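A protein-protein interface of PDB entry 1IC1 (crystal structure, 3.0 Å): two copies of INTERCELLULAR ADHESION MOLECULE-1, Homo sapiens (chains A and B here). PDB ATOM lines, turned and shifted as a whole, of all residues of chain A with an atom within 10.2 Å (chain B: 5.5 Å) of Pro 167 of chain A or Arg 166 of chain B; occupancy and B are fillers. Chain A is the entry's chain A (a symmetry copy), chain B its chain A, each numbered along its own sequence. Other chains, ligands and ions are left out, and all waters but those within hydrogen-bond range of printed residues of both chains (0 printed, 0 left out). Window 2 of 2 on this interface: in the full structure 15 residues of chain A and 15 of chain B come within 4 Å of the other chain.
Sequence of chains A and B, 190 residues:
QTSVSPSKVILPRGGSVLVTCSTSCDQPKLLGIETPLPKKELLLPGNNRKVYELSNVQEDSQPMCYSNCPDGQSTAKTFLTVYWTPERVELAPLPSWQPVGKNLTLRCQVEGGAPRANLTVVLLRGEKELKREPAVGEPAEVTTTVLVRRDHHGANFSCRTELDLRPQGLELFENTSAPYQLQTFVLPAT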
ATOM      1  N   LYS A   8     -35.028  -8.786 -27.695  1.00  0.00           N
ATOM      2  CA  LYS A   8     -34.006  -8.046 -28.362  1.00  0.00           C
ATOM      3  C   LYS A   8     -32.960  -9.113 -28.604  1.00  0.00           C
ATOM      4  O   LYS A   8     -32.797 -10.009 -27.762  1.00  0.00           O
ATOM      5  CB  LYS A   8     -33.477  -6.932 -27.446  1.00  0.00           C
ATOM      6  CG  LYS A   8     -32.576  -5.925 -28.179  1.00  0.00           C
ATOM      7  CD  LYS A   8     -31.099  -6.435 -28.348  1.00  0.00           C
ATOM      8  CE  LYS A   8     -30.290  -5.722 -29.500  1.00  0.00           C
ATOM      9  NZ  LYS A   8     -29.106  -4.855 -29.044  1.00  0.00           N
ATOM     10  N   ILE A  10     -28.956  -9.579 -30.736  1.00  0.00           N
ATOM     11  CA  ILE A  10     -27.883  -9.024 -31.533  1.00  0.00           C
ATOM     12  C   ILE A  10     -27.237 -10.256 -32.174  1.00  0.00           C
ATOM     13  O   ILE A  10     -26.846 -11.219 -31.474  1.00  0.00           O
ATOM     14  CB  ILE A  10     -26.876  -8.167 -30.615  1.00  0.00           C
ATOM     15  CG1 ILE A  10     -26.378  -6.875 -31.345  1.00  0.00           C
ATOM     16  CG2 ILE A  10     -25.748  -9.055 -29.975  1.00  0.00           C
ATOM     17  CD1 ILE A  10     -25.595  -7.075 -32.604  1.00  0.00           C
ATOM     18  N   PRO A 115     -24.929  -2.455 -37.306  1.00  0.00           N
ATOM     19  CA  PRO A 115     -25.914  -1.374 -37.384  1.00  0.00           C
ATOM     20  C   PRO A 115     -25.234  -0.034 -37.376  1.00  0.00           C
ATOM     21  O   PRO A 115     -24.467   0.282 -36.446  1.00  0.00           O
ATOM     22  CB  PRO A 115     -26.721  -1.573 -36.111  1.00  0.00           C
ATOM     23  CG  PRO A 115     -25.698  -1.931 -35.162  1.00  0.00           C
ATOM     24  CD  PRO A 115     -24.818  -2.928 -35.919  1.00  0.00           C
ATOM     25  N   ALA A 117     -26.128   2.657 -36.535  1.00  0.00           N
ATOM     26  CA  ALA A 117     -26.295   3.468 -35.360  1.00  0.00           C
ATOM     27  C   ALA A 117     -25.079   3.361 -34.435  1.00  0.00           C
ATOM     28  O   ALA A 117     -24.773   4.331 -33.757  1.00  0.00           O
ATOM     29  CB  ALA A 117     -27.534   3.121 -34.659  1.00  0.00           C
ATOM     30  N   ASN A 118     -24.384   2.217 -34.409  1.00  0.00           N
ATOM     31  CA  ASN A 118     -23.164   2.068 -33.578  1.00  0.00           C
ATOM     32  C   ASN A 118     -21.869   2.189 -34.384  1.00  0.00           C
ATOM     33  O   ASN A 118     -20.777   1.794 -33.918  1.00  0.00           O
ATOM     34  CB  ASN A 118     -23.046   0.695 -32.979  1.00  0.00           C
ATOM     35  CG  ASN A 118     -24.161   0.360 -32.105  1.00  0.00           C
ATOM     36  OD1 ASN A 118     -24.990  -0.470 -32.472  1.00  0.00           O
ATOM     37  ND2 ASN A 118     -24.209   0.961 -30.924  1.00  0.00           N
ATOM     38  N   LEU A 119     -21.987   2.603 -35.630  1.00  0.00           N
ATOM     39  CA  LEU A 119     -20.796   2.694 -36.423  1.00  0.00           C
ATOM     40  C   LEU A 119     -20.313   4.118 -36.482  1.00  0.00           C
ATOM     41  O   LEU A 119     -21.035   4.998 -36.973  1.00  0.00           O
ATOM     42  CB  LEU A 119     -21.046   2.174 -37.830  1.00  0.00           C
ATOM     43  CG  LEU A 119     -19.762   1.750 -38.571  1.00  0.00           C
ATOM     44  CD1 LEU A 119     -19.164   0.497 -38.004  1.00  0.00           C
ATOM     45  CD2 LEU A 119     -20.106   1.492 -40.000  1.00  0.00           C
ATOM     46  N   GLU A 162     -15.412   2.340 -36.079  1.00  0.00           N
ATOM     47  CA  GLU A 162     -15.644   1.732 -34.789  1.00  0.00           C
ATOM     48  C   GLU A 162     -17.060   1.231 -34.679  1.00  0.00           C
ATOM     49  O   GLU A 162     -17.999   2.060 -34.654  1.00  0.00           O
ATOM     50  CB  GLU A 162     -15.418   2.763 -33.685  1.00  0.00           C
ATOM     51  CG  GLU A 162     -13.992   3.308 -33.593  1.00  0.00           C
ATOM     52  CD  GLU A 162     -13.852   4.401 -32.544  1.00  0.00           C
ATOM     53  OE1 GLU A 162     -14.885   4.741 -31.953  1.00  0.00           O
ATOM     54  OE2 GLU A 162     -12.740   4.944 -32.324  1.00  0.00           O
ATOM     55  N   LEU A 163     -17.205  -0.106 -34.621  1.00  0.00           N
ATOM     56  CA  LEU A 163     -18.507  -0.788 -34.479  1.00  0.00           C
ATOM     57  C   LEU A 163     -18.632  -1.255 -33.044  1.00  0.00           C
ATOM     58  O   LEU A 163     -18.276  -2.390 -32.693  1.00  0.00           O
ATOM     59  CB  LEU A 163     -18.627  -1.995 -35.397  1.00  0.00           C
ATOM     60  CG  LEU A 163     -20.040  -2.574 -35.372  1.00  0.00           C
ATOM     61  CD1 LEU A 163     -21.117  -1.584 -35.896  1.00  0.00           C
ATOM     62  CD2 LEU A 163     -20.040  -3.822 -36.184  1.00  0.00           C
ATOM     63  N   ASP A 164     -19.201  -0.375 -32.227  1.00  0.00           N
ATOM     64  CA  ASP A 164     -19.348  -0.629 -30.808  1.00  0.00           C
ATOM     65  C   ASP A 164     -20.548  -1.445 -30.394  1.00  0.00           C
ATOM     66  O   ASP A 164     -21.649  -0.926 -30.152  1.00  0.00           O
ATOM     67  CB  ASP A 164     -19.364   0.685 -30.069  1.00  0.00           C
ATOM     68  CG  ASP A 164     -18.745   0.588 -28.719  1.00  0.00           C
ATOM     69  OD1 ASP A 164     -18.977  -0.391 -27.984  1.00  0.00           O
ATOM     70  OD2 ASP A 164     -18.017   1.529 -28.394  1.00  0.00           O
ATOM     71  N   LEU A 165     -20.304  -2.729 -30.235  1.00  0.00           N
ATOM     72  CA  LEU A 165     -21.362  -3.626 -29.795  1.00  0.00           C
ATOM     73  C   LEU A 165     -21.110  -4.030 -28.338  1.00  0.00           C
ATOM     74  O   LEU A 165     -21.611  -5.026 -27.858  1.00  0.00           O
ATOM     75  CB  LEU A 165     -21.455  -4.843 -30.729  1.00  0.00           C
ATOM     76  CG  LEU A 165     -21.603  -4.415 -32.192  1.00  0.00           C
ATOM     77  CD1 LEU A 165     -21.846  -5.599 -33.052  1.00  0.00           C
ATOM     78  CD2 LEU A 165     -22.746  -3.398 -32.326  1.00  0.00           C
ATOM     79  N   ARG A 166     -20.365  -3.211 -27.629  1.00  0.00           N
ATOM     80  CA  ARG A 166     -20.094  -3.495 -26.250  1.00  0.00           C
ATOM     81  C   ARG A 166     -21.354  -3.359 -25.412  1.00  0.00           C
ATOM     82  O   ARG A 166     -21.695  -4.264 -24.638  1.00  0.00           O
ATOM     83  CB  ARG A 166     -19.030  -2.548 -25.708  1.00  0.00           C
ATOM     84  CG  ARG A 166     -17.701  -2.698 -26.374  1.00  0.00           C
ATOM     85  CD  ARG A 166     -16.662  -1.881 -25.678  1.00  0.00           C
ATOM     86  NE  ARG A 166     -16.734  -0.461 -25.989  1.00  0.00           N
ATOM     87  CZ  ARG A 166     -15.883   0.419 -25.478  1.00  0.00           C
ATOM     88  NH1 ARG A 166     -14.915   0.017 -24.662  1.00  0.00           N
ATOM     89  NH2 ARG A 166     -16.021   1.705 -25.721  1.00  0.00           N
ATOM     90  N   PRO A 167     -22.072  -2.227 -25.541  1.00  0.00           N
ATOM     91  CA  PRO A 167     -23.284  -2.091 -24.732  1.00  0.00           C
ATOM     92  C   PRO A 167     -24.337  -3.148 -25.070  1.00  0.00           C
ATOM     93  O   PRO A 167     -25.256  -3.397 -24.303  1.00  0.00           O
ATOM     94  CB  PRO A 167     -23.732  -0.680 -25.054  1.00  0.00           C
ATOM     95  CG  PRO A 167     -23.229  -0.481 -26.460  1.00  0.00           C
ATOM     96  CD  PRO A 167     -21.857  -1.020 -26.353  1.00  0.00           C
ATOM     97  N   GLN A 168     -24.166  -3.820 -26.192  1.00  0.00           N
ATOM     98  CA  GLN A 168     -25.129  -4.826 -26.556  1.00  0.00           C
ATOM     99  C   GLN A 168     -24.600  -6.174 -26.137  1.00  0.00           C
ATOM    100  O   GLN A 168     -25.132  -7.198 -26.504  1.00  0.00           O
ATOM    101  CB  GLN A 168     -25.372  -4.780 -28.053  1.00  0.00           C
ATOM    102  CG  GLN A 168     -24.854  -3.497 -28.729  1.00  0.00           C
ATOM    103  CD  GLN A 168     -25.838  -2.911 -29.734  1.00  0.00           C
ATOM    104  OE1 GLN A 168     -26.966  -3.402 -29.905  1.00  0.00           O
ATOM    105  NE2 GLN A 168     -25.430  -1.827 -30.370  1.00  0.00           N
ATOM    106  N   GLY A 169     -23.542  -6.167 -25.344  1.00  0.00           N
ATOM    107  CA  GLY A 169     -22.957  -7.417 -24.887  1.00  0.00           C
ATOM    108  C   GLY A 169     -21.771  -7.928 -25.715  1.00  0.00           C
ATOM    109  O   GLY A 169     -21.002  -8.801 -25.258  1.00  0.00           O
ATOM    110  N   LEU A 170     -21.592  -7.400 -26.925  1.00  0.00           N
ATOM    111  CA  LEU A 170     -20.491  -7.860 -27.769  1.00  0.00           C
ATOM    112  C   LEU A 170     -19.174  -7.116 -27.550  1.00  0.00           C
ATOM    113  O   LEU A 170     -18.708  -6.974 -26.432  1.00  0.00           O
ATOM    114  CB  LEU A 170     -20.895  -7.853 -29.256  1.00  0.00           C
ATOM    115  CG  LEU A 170     -22.079  -8.737 -29.633  1.00  0.00           C
ATOM    116  CD1 LEU A 170     -22.270  -8.725 -31.109  1.00  0.00           C
ATOM    117  CD2 LEU A 170     -21.801 -10.132 -29.190  1.00  0.00           C
ATOM    118  N   GLU A 171     -18.548  -6.700 -28.641  1.00  0.00           N
ATOM    119  CA  GLU A 171     -17.300  -5.999 -28.553  1.00  0.00           C
ATOM    120  C   GLU A 171     -17.386  -4.720 -29.364  1.00  0.00           C
ATOM    121  O   GLU A 171     -18.431  -4.332 -29.888  1.00  0.00           O
ATOM    122  CB  GLU A 171     -16.191  -6.838 -29.171  1.00  0.00           C
ATOM    123  CG  GLU A 171     -16.309  -8.344 -29.047  1.00  0.00           C
ATOM    124  CD  GLU A 171     -15.147  -9.098 -29.749  1.00  0.00           C
ATOM    125  OE1 GLU A 171     -14.450  -8.506 -30.613  1.00  0.00           O
ATOM    126  OE2 GLU A 171     -14.928 -10.295 -29.447  1.00  0.00           O
ATOM    127  N   LEU A 172     -16.241  -4.062 -29.457  1.00  0.00           N
ATOM    128  CA  LEU A 172     -16.086  -2.859 -30.264  1.00  0.00           C
ATOM    129  C   LEU A 172     -15.270  -3.344 -31.480  1.00  0.00           C
ATOM    130  O   LEU A 172     -14.121  -3.717 -31.348  1.00  0.00           O
ATOM    131  CB  LEU A 172     -15.261  -1.841 -29.499  1.00  0.00           C
ATOM    132  CG  LEU A 172     -14.778  -0.749 -30.456  1.00  0.00           C
ATOM    133  CD1 LEU A 172     -15.992   0.092 -30.944  1.00  0.00           C
ATOM    134  CD2 LEU A 172     -13.712   0.100 -29.771  1.00  0.00           C
ATOM    135  N   PHE A 173     -15.849  -3.371 -32.657  1.00  0.00           N
ATOM    136  CA  PHE A 173     -15.097  -3.865 -33.788  1.00  0.00           C
ATOM    137  C   PHE A 173     -14.519  -2.727 -34.619  1.00  0.00           C
ATOM    138  O   PHE A 173     -15.258  -1.849 -35.073  1.00  0.00           O
ATOM    139  CB  PHE A 173     -15.995  -4.769 -34.646  1.00  0.00           C
ATOM    140  CG  PHE A 173     -16.620  -5.876 -33.884  1.00  0.00           C
ATOM    141  CD1 PHE A 173     -15.905  -7.047 -33.619  1.00  0.00           C
ATOM    142  CD2 PHE A 173     -17.920  -5.755 -33.405  1.00  0.00           C
ATOM    143  CE1 PHE A 173     -16.478  -8.099 -32.891  1.00  0.00           C
ATOM    144  CE2 PHE A 173     -18.507  -6.804 -32.670  1.00  0.00           C
ATOM    145  CZ  PHE A 173     -17.777  -7.972 -32.416  1.00  0.00           C
ATOM    146  N   ASP B 164     -23.459  -4.301 -11.967  1.00  0.00           N
ATOM    147  CA  ASP B 164     -23.210  -3.891 -13.335  1.00  0.00           C
ATOM    148  C   ASP B 164     -23.258  -4.978 -14.379  1.00  0.00           C
ATOM    149  O   ASP B 164     -22.261  -5.656 -14.675  1.00  0.00           O
ATOM    150  CB  ASP B 164     -21.875  -3.193 -13.407  1.00  0.00           C
ATOM    151  CG  ASP B 164     -21.851  -2.113 -14.431  1.00  0.00           C
ATOM    152  OD1 ASP B 164     -22.374  -2.287 -15.548  1.00  0.00           O
ATOM    153  OD2 ASP B 164     -21.280  -1.072 -14.099  1.00  0.00           O
ATOM    154  N   LEU B 165     -24.414  -5.086 -15.001  1.00  0.00           N
ATOM    155  CA  LEU B 165     -24.586  -6.066 -16.062  1.00  0.00           C
ATOM    156  C   LEU B 165     -24.630  -5.344 -17.414  1.00  0.00           C
ATOM    157  O   LEU B 165     -25.121  -5.863 -18.396  1.00  0.00           O
ATOM    158  CB  LEU B 165     -25.844  -6.911 -15.812  1.00  0.00           C
ATOM    159  CG  LEU B 165     -25.828  -7.540 -14.416  1.00  0.00           C
ATOM    160  CD1 LEU B 165     -26.971  -8.471 -14.257  1.00  0.00           C
ATOM    161  CD2 LEU B 165     -24.494  -8.266 -14.185  1.00  0.00           C
ATOM    162  N   ARG B 166     -24.061  -4.160 -17.460  1.00  0.00           N
ATOM    163  CA  ARG B 166     -24.034  -3.420 -18.686  1.00  0.00           C
ATOM    164  C   ARG B 166     -23.125  -4.091 -19.703  1.00  0.00           C
ATOM    165  O   ARG B 166     -23.527  -4.319 -20.852  1.00  0.00           O
ATOM    166  CB  ARG B 166     -23.544  -1.998 -18.443  1.00  0.00           C
ATOM    167  CG  ARG B 166     -24.448  -1.197 -17.562  1.00  0.00           C
ATOM    168  CD  ARG B 166     -24.015   0.231 -17.513  1.00  0.00           C
ATOM    169  NE  ARG B 166     -22.863   0.460 -16.655  1.00  0.00           N
ATOM    170  CZ  ARG B 166     -22.345   1.669 -16.475  1.00  0.00           C
ATOM    171  NH1 ARG B 166     -22.885   2.724 -17.074  1.00  0.00           N
ATOM    172  NH2 ARG B 166     -21.258   1.831 -15.751  1.00  0.00           N
ATOM    173  N   PRO B 167     -21.880  -4.420 -19.307  1.00  0.00           N
ATOM    174  CA  PRO B 167     -21.000  -5.062 -20.284  1.00  0.00           C
ATOM    175  C   PRO B 167     -21.530  -6.421 -20.747  1.00  0.00           C
ATOM    176  O   PRO B 167     -21.120  -6.948 -21.771  1.00  0.00           O
ATOM    177  CB  PRO B 167     -19.691  -5.160 -19.526  1.00  0.00           C
ATOM    178  CG  PRO B 167     -20.141  -5.278 -18.094  1.00  0.00           C
ATOM    179  CD  PRO B 167     -21.176  -4.225 -18.030  1.00  0.00           C
ATOM    180  N   GLN B 168     -22.495  -6.960 -20.026  1.00  0.00           N
ATOM    181  CA  GLN B 168     -23.028  -8.237 -20.419  1.00  0.00           C
ATOM    182  C   GLN B 168     -24.291  -8.009 -21.210  1.00  0.00           C
ATOM    183  O   GLN B 168     -25.032  -8.927 -21.487  1.00  0.00           O
ATOM    184  CB  GLN B 168     -23.304  -9.075 -19.184  1.00  0.00           C
ATOM    185  CG  GLN B 168     -22.631  -8.541 -17.906  1.00  0.00           C
ATOM    186  CD  GLN B 168     -21.981  -9.636 -17.070  1.00  0.00           C
ATOM    187  OE1 GLN B 168     -21.949 -10.818 -17.454  1.00  0.00           O
ATOM    188  NE2 GLN B 168     -21.418  -9.238 -15.943  1.00  0.00           N
ATOM    189  N   GLY B 169     -24.529  -6.765 -21.587  1.00  0.00           N
ATOM    190  CA  GLY B 169     -25.723  -6.444 -22.353  1.00  0.00           C
ATOM    191  C   GLY B 169     -26.916  -5.944 -21.529  1.00  0.00           C
ATOM    192  O   GLY B 169     -27.870  -5.353 -22.079  1.00  0.00           O
ATOM    193  N   LEU B 170     -26.887  -6.154 -20.213  1.00  0.00           N
ATOM    194  CA  LEU B 170     -28.004  -5.719 -19.377  1.00  0.00           C
ATOM    195  C   LEU B 170     -27.891  -4.280 -18.872  1.00  0.00           C
ATOM    196  O   LEU B 170     -27.661  -3.359 -19.638  1.00  0.00           O
ATOM    197  CB  LEU B 170     -28.239  -6.701 -18.213  1.00  0.00           C
ATOM    198  CG  LEU B 170     -28.575  -8.136 -18.605  1.00  0.00           C
ATOM    199  CD1 LEU B 170     -28.897  -8.930 -17.388  1.00  0.00           C
ATOM    200  CD2 LEU B 170     -29.761  -8.126 -19.508  1.00  0.00           C
ATOM    201  N   GLU B 171     -28.121  -4.093 -17.582  1.00  0.00           N
ATOM    202  CA  GLU B 171     -28.051  -2.782 -17.003  1.00  0.00           C
ATOM    203  C   GLU B 171     -27.152  -2.822 -15.781  1.00  0.00           C
ATOM    204  O   GLU B 171     -26.509  -3.822 -15.460  1.00  0.00           O
ATOM    205  CB  GLU B 171     -29.430  -2.356 -16.521  1.00  0.00           C
ATOM    206  CG  GLU B 171     -30.625  -2.854 -17.309  1.00  0.00           C
ATOM    207  CD  GLU B 171     -31.979  -2.392 -16.704  1.00  0.00           C
ATOM    208  OE1 GLU B 171     -32.027  -1.994 -15.512  1.00  0.00           O
ATOM    209  OE2 GLU B 171     -33.010  -2.434 -17.417  1.00  0.00           O
ATOM    210  N   LEU B 172     -27.125  -1.691 -15.095  1.00  0.00           N
ATOM    211  CA  LEU B 172     -26.397  -1.546 -13.841  1.00  0.00           C
ATOM    212  C   LEU B 172     -27.513  -1.521 -12.777  1.00  0.00           C
ATOM    213  O   LEU B 172     -28.302  -0.596 -12.727  1.00  0.00           O
ATOM    214  CB  LEU B 172     -25.679  -0.209 -13.825  1.00  0.00           C
ATOM    215  CG  LEU B 172     -25.233   0.116 -12.398  1.00  0.00           C
ATOM    216  CD1 LEU B 172     -24.118  -0.876 -11.960  1.00  0.00           C
ATOM    217  CD2 LEU B 172     -24.788   1.573 -12.319  1.00  0.00           C
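O of Pro 167 of chain B touches O of Arg 166 of chain A (3.97 Å). Pro 167 of chain A touches Arg 166 of chain B (O to O, 3.97 Å). O of Pro 167 of chain A touches CA of Gly 169 of chain B (3.6 Å). C of Gln 168 of chain A touches CA of Gly 169 of chain B (3.96 Å). Gly 169 of chain A touches Pro 167 of chain B (CA to O, 3.6 Å). Gln 168 of chain B touches Gly 169 of chain A (C to CA, 3.96 Å). N of Gly 169 of chain A touches CA of Gly 169 of chain B, at 3.7 Å.
The side-chain carboxylate of Asp 164 of chain B lies within salt-bridge range of the guanidinium group of Arg 166 of chain B, 3.0 Å away. N of Arg 166 of chain B sits at hydrogen-bond distance from O of Glu 171 of chain B. The side-chain amino group (NZ) of Lys 8 of chain A sits at hydrogen-bond distance from the side-chain amide oxygen (OE1) of Gln 168 of chain A (2.7 Å). OD1 of Asn 118 of chain A lies within hydrogen-bond range of NE2 of Gln 168 of chain A (2.5 Å). OD1 of Asp 164 of chain A lies within salt-bridge range of NE of Arg 166 of chain A (3.0 Å). The backbone carbonyl oxygen (O) of Glu 171 of chain A lies within hydrogen-bond range of the backbone NH (N) of Arg 166 of chain A, at 3.2 Å.
Printed residues of chain A that touch a printed residue of chain B: Arg 166, Pro 167, Gln 168 and Gly 169.
Arg 166 of chain A touches Pro 167 of chain B, and with the chains exchanged Pro 167 of chain A touches Arg 166 of chain B. Pro 167 of chain A touches Gly 169 of chain B, and with the chains exchanged Gly 169 of chain A touches Pro 167 of chain B. Gln 168 of chain A touches Gly 169 of chain B, and with the chains exchanged Gly 169 of chain A touches Gln 168 of chain B. Gly 169 of chain A touches its own counterpart, Gly 169 of chain B. Positions printed for both chains: 164, 165, 166, 167, 168, 169, 170, 171 and 172.
Printed residues of chain B within 4 Å of Arg 166 of chain A: Pro 167 (3.97 Å). Of chain B, only Arg 166 and Gly 169 come within 4 Å of Pro 167 of chain A. Of the printed residues of chain B, Gln 168 of chain A touches Gly 169 (3.96 Å). Printed residues of chain B within 4 Å of Gly 169 of chain A: Pro 167 (3.6 Å), Gln 168 (3.96 Å) and Gly 169 (3.7 Å). Asp 164 of chain B touches none of the printed residues of chain A. Leu 165 of chain B touches none of the printed residues of chain A. Of chain A, only Pro 167 comes within 4 Å of Arg 166 of chain B. Of chain A, only Pro 167, Gln 168 and Gly 169 come within 4 Å of Gly 169 of chain B. Leu 170 of chain B touches none of the printed residues of chain A. The nearest residue of chain B that does not touch Pro 167 of chain A is Leu 170 of chain B (5.2 Å). The nearest residue of chain A that does not touch Arg 166 of chain B is Arg 166 of chain A (4.2 Å).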
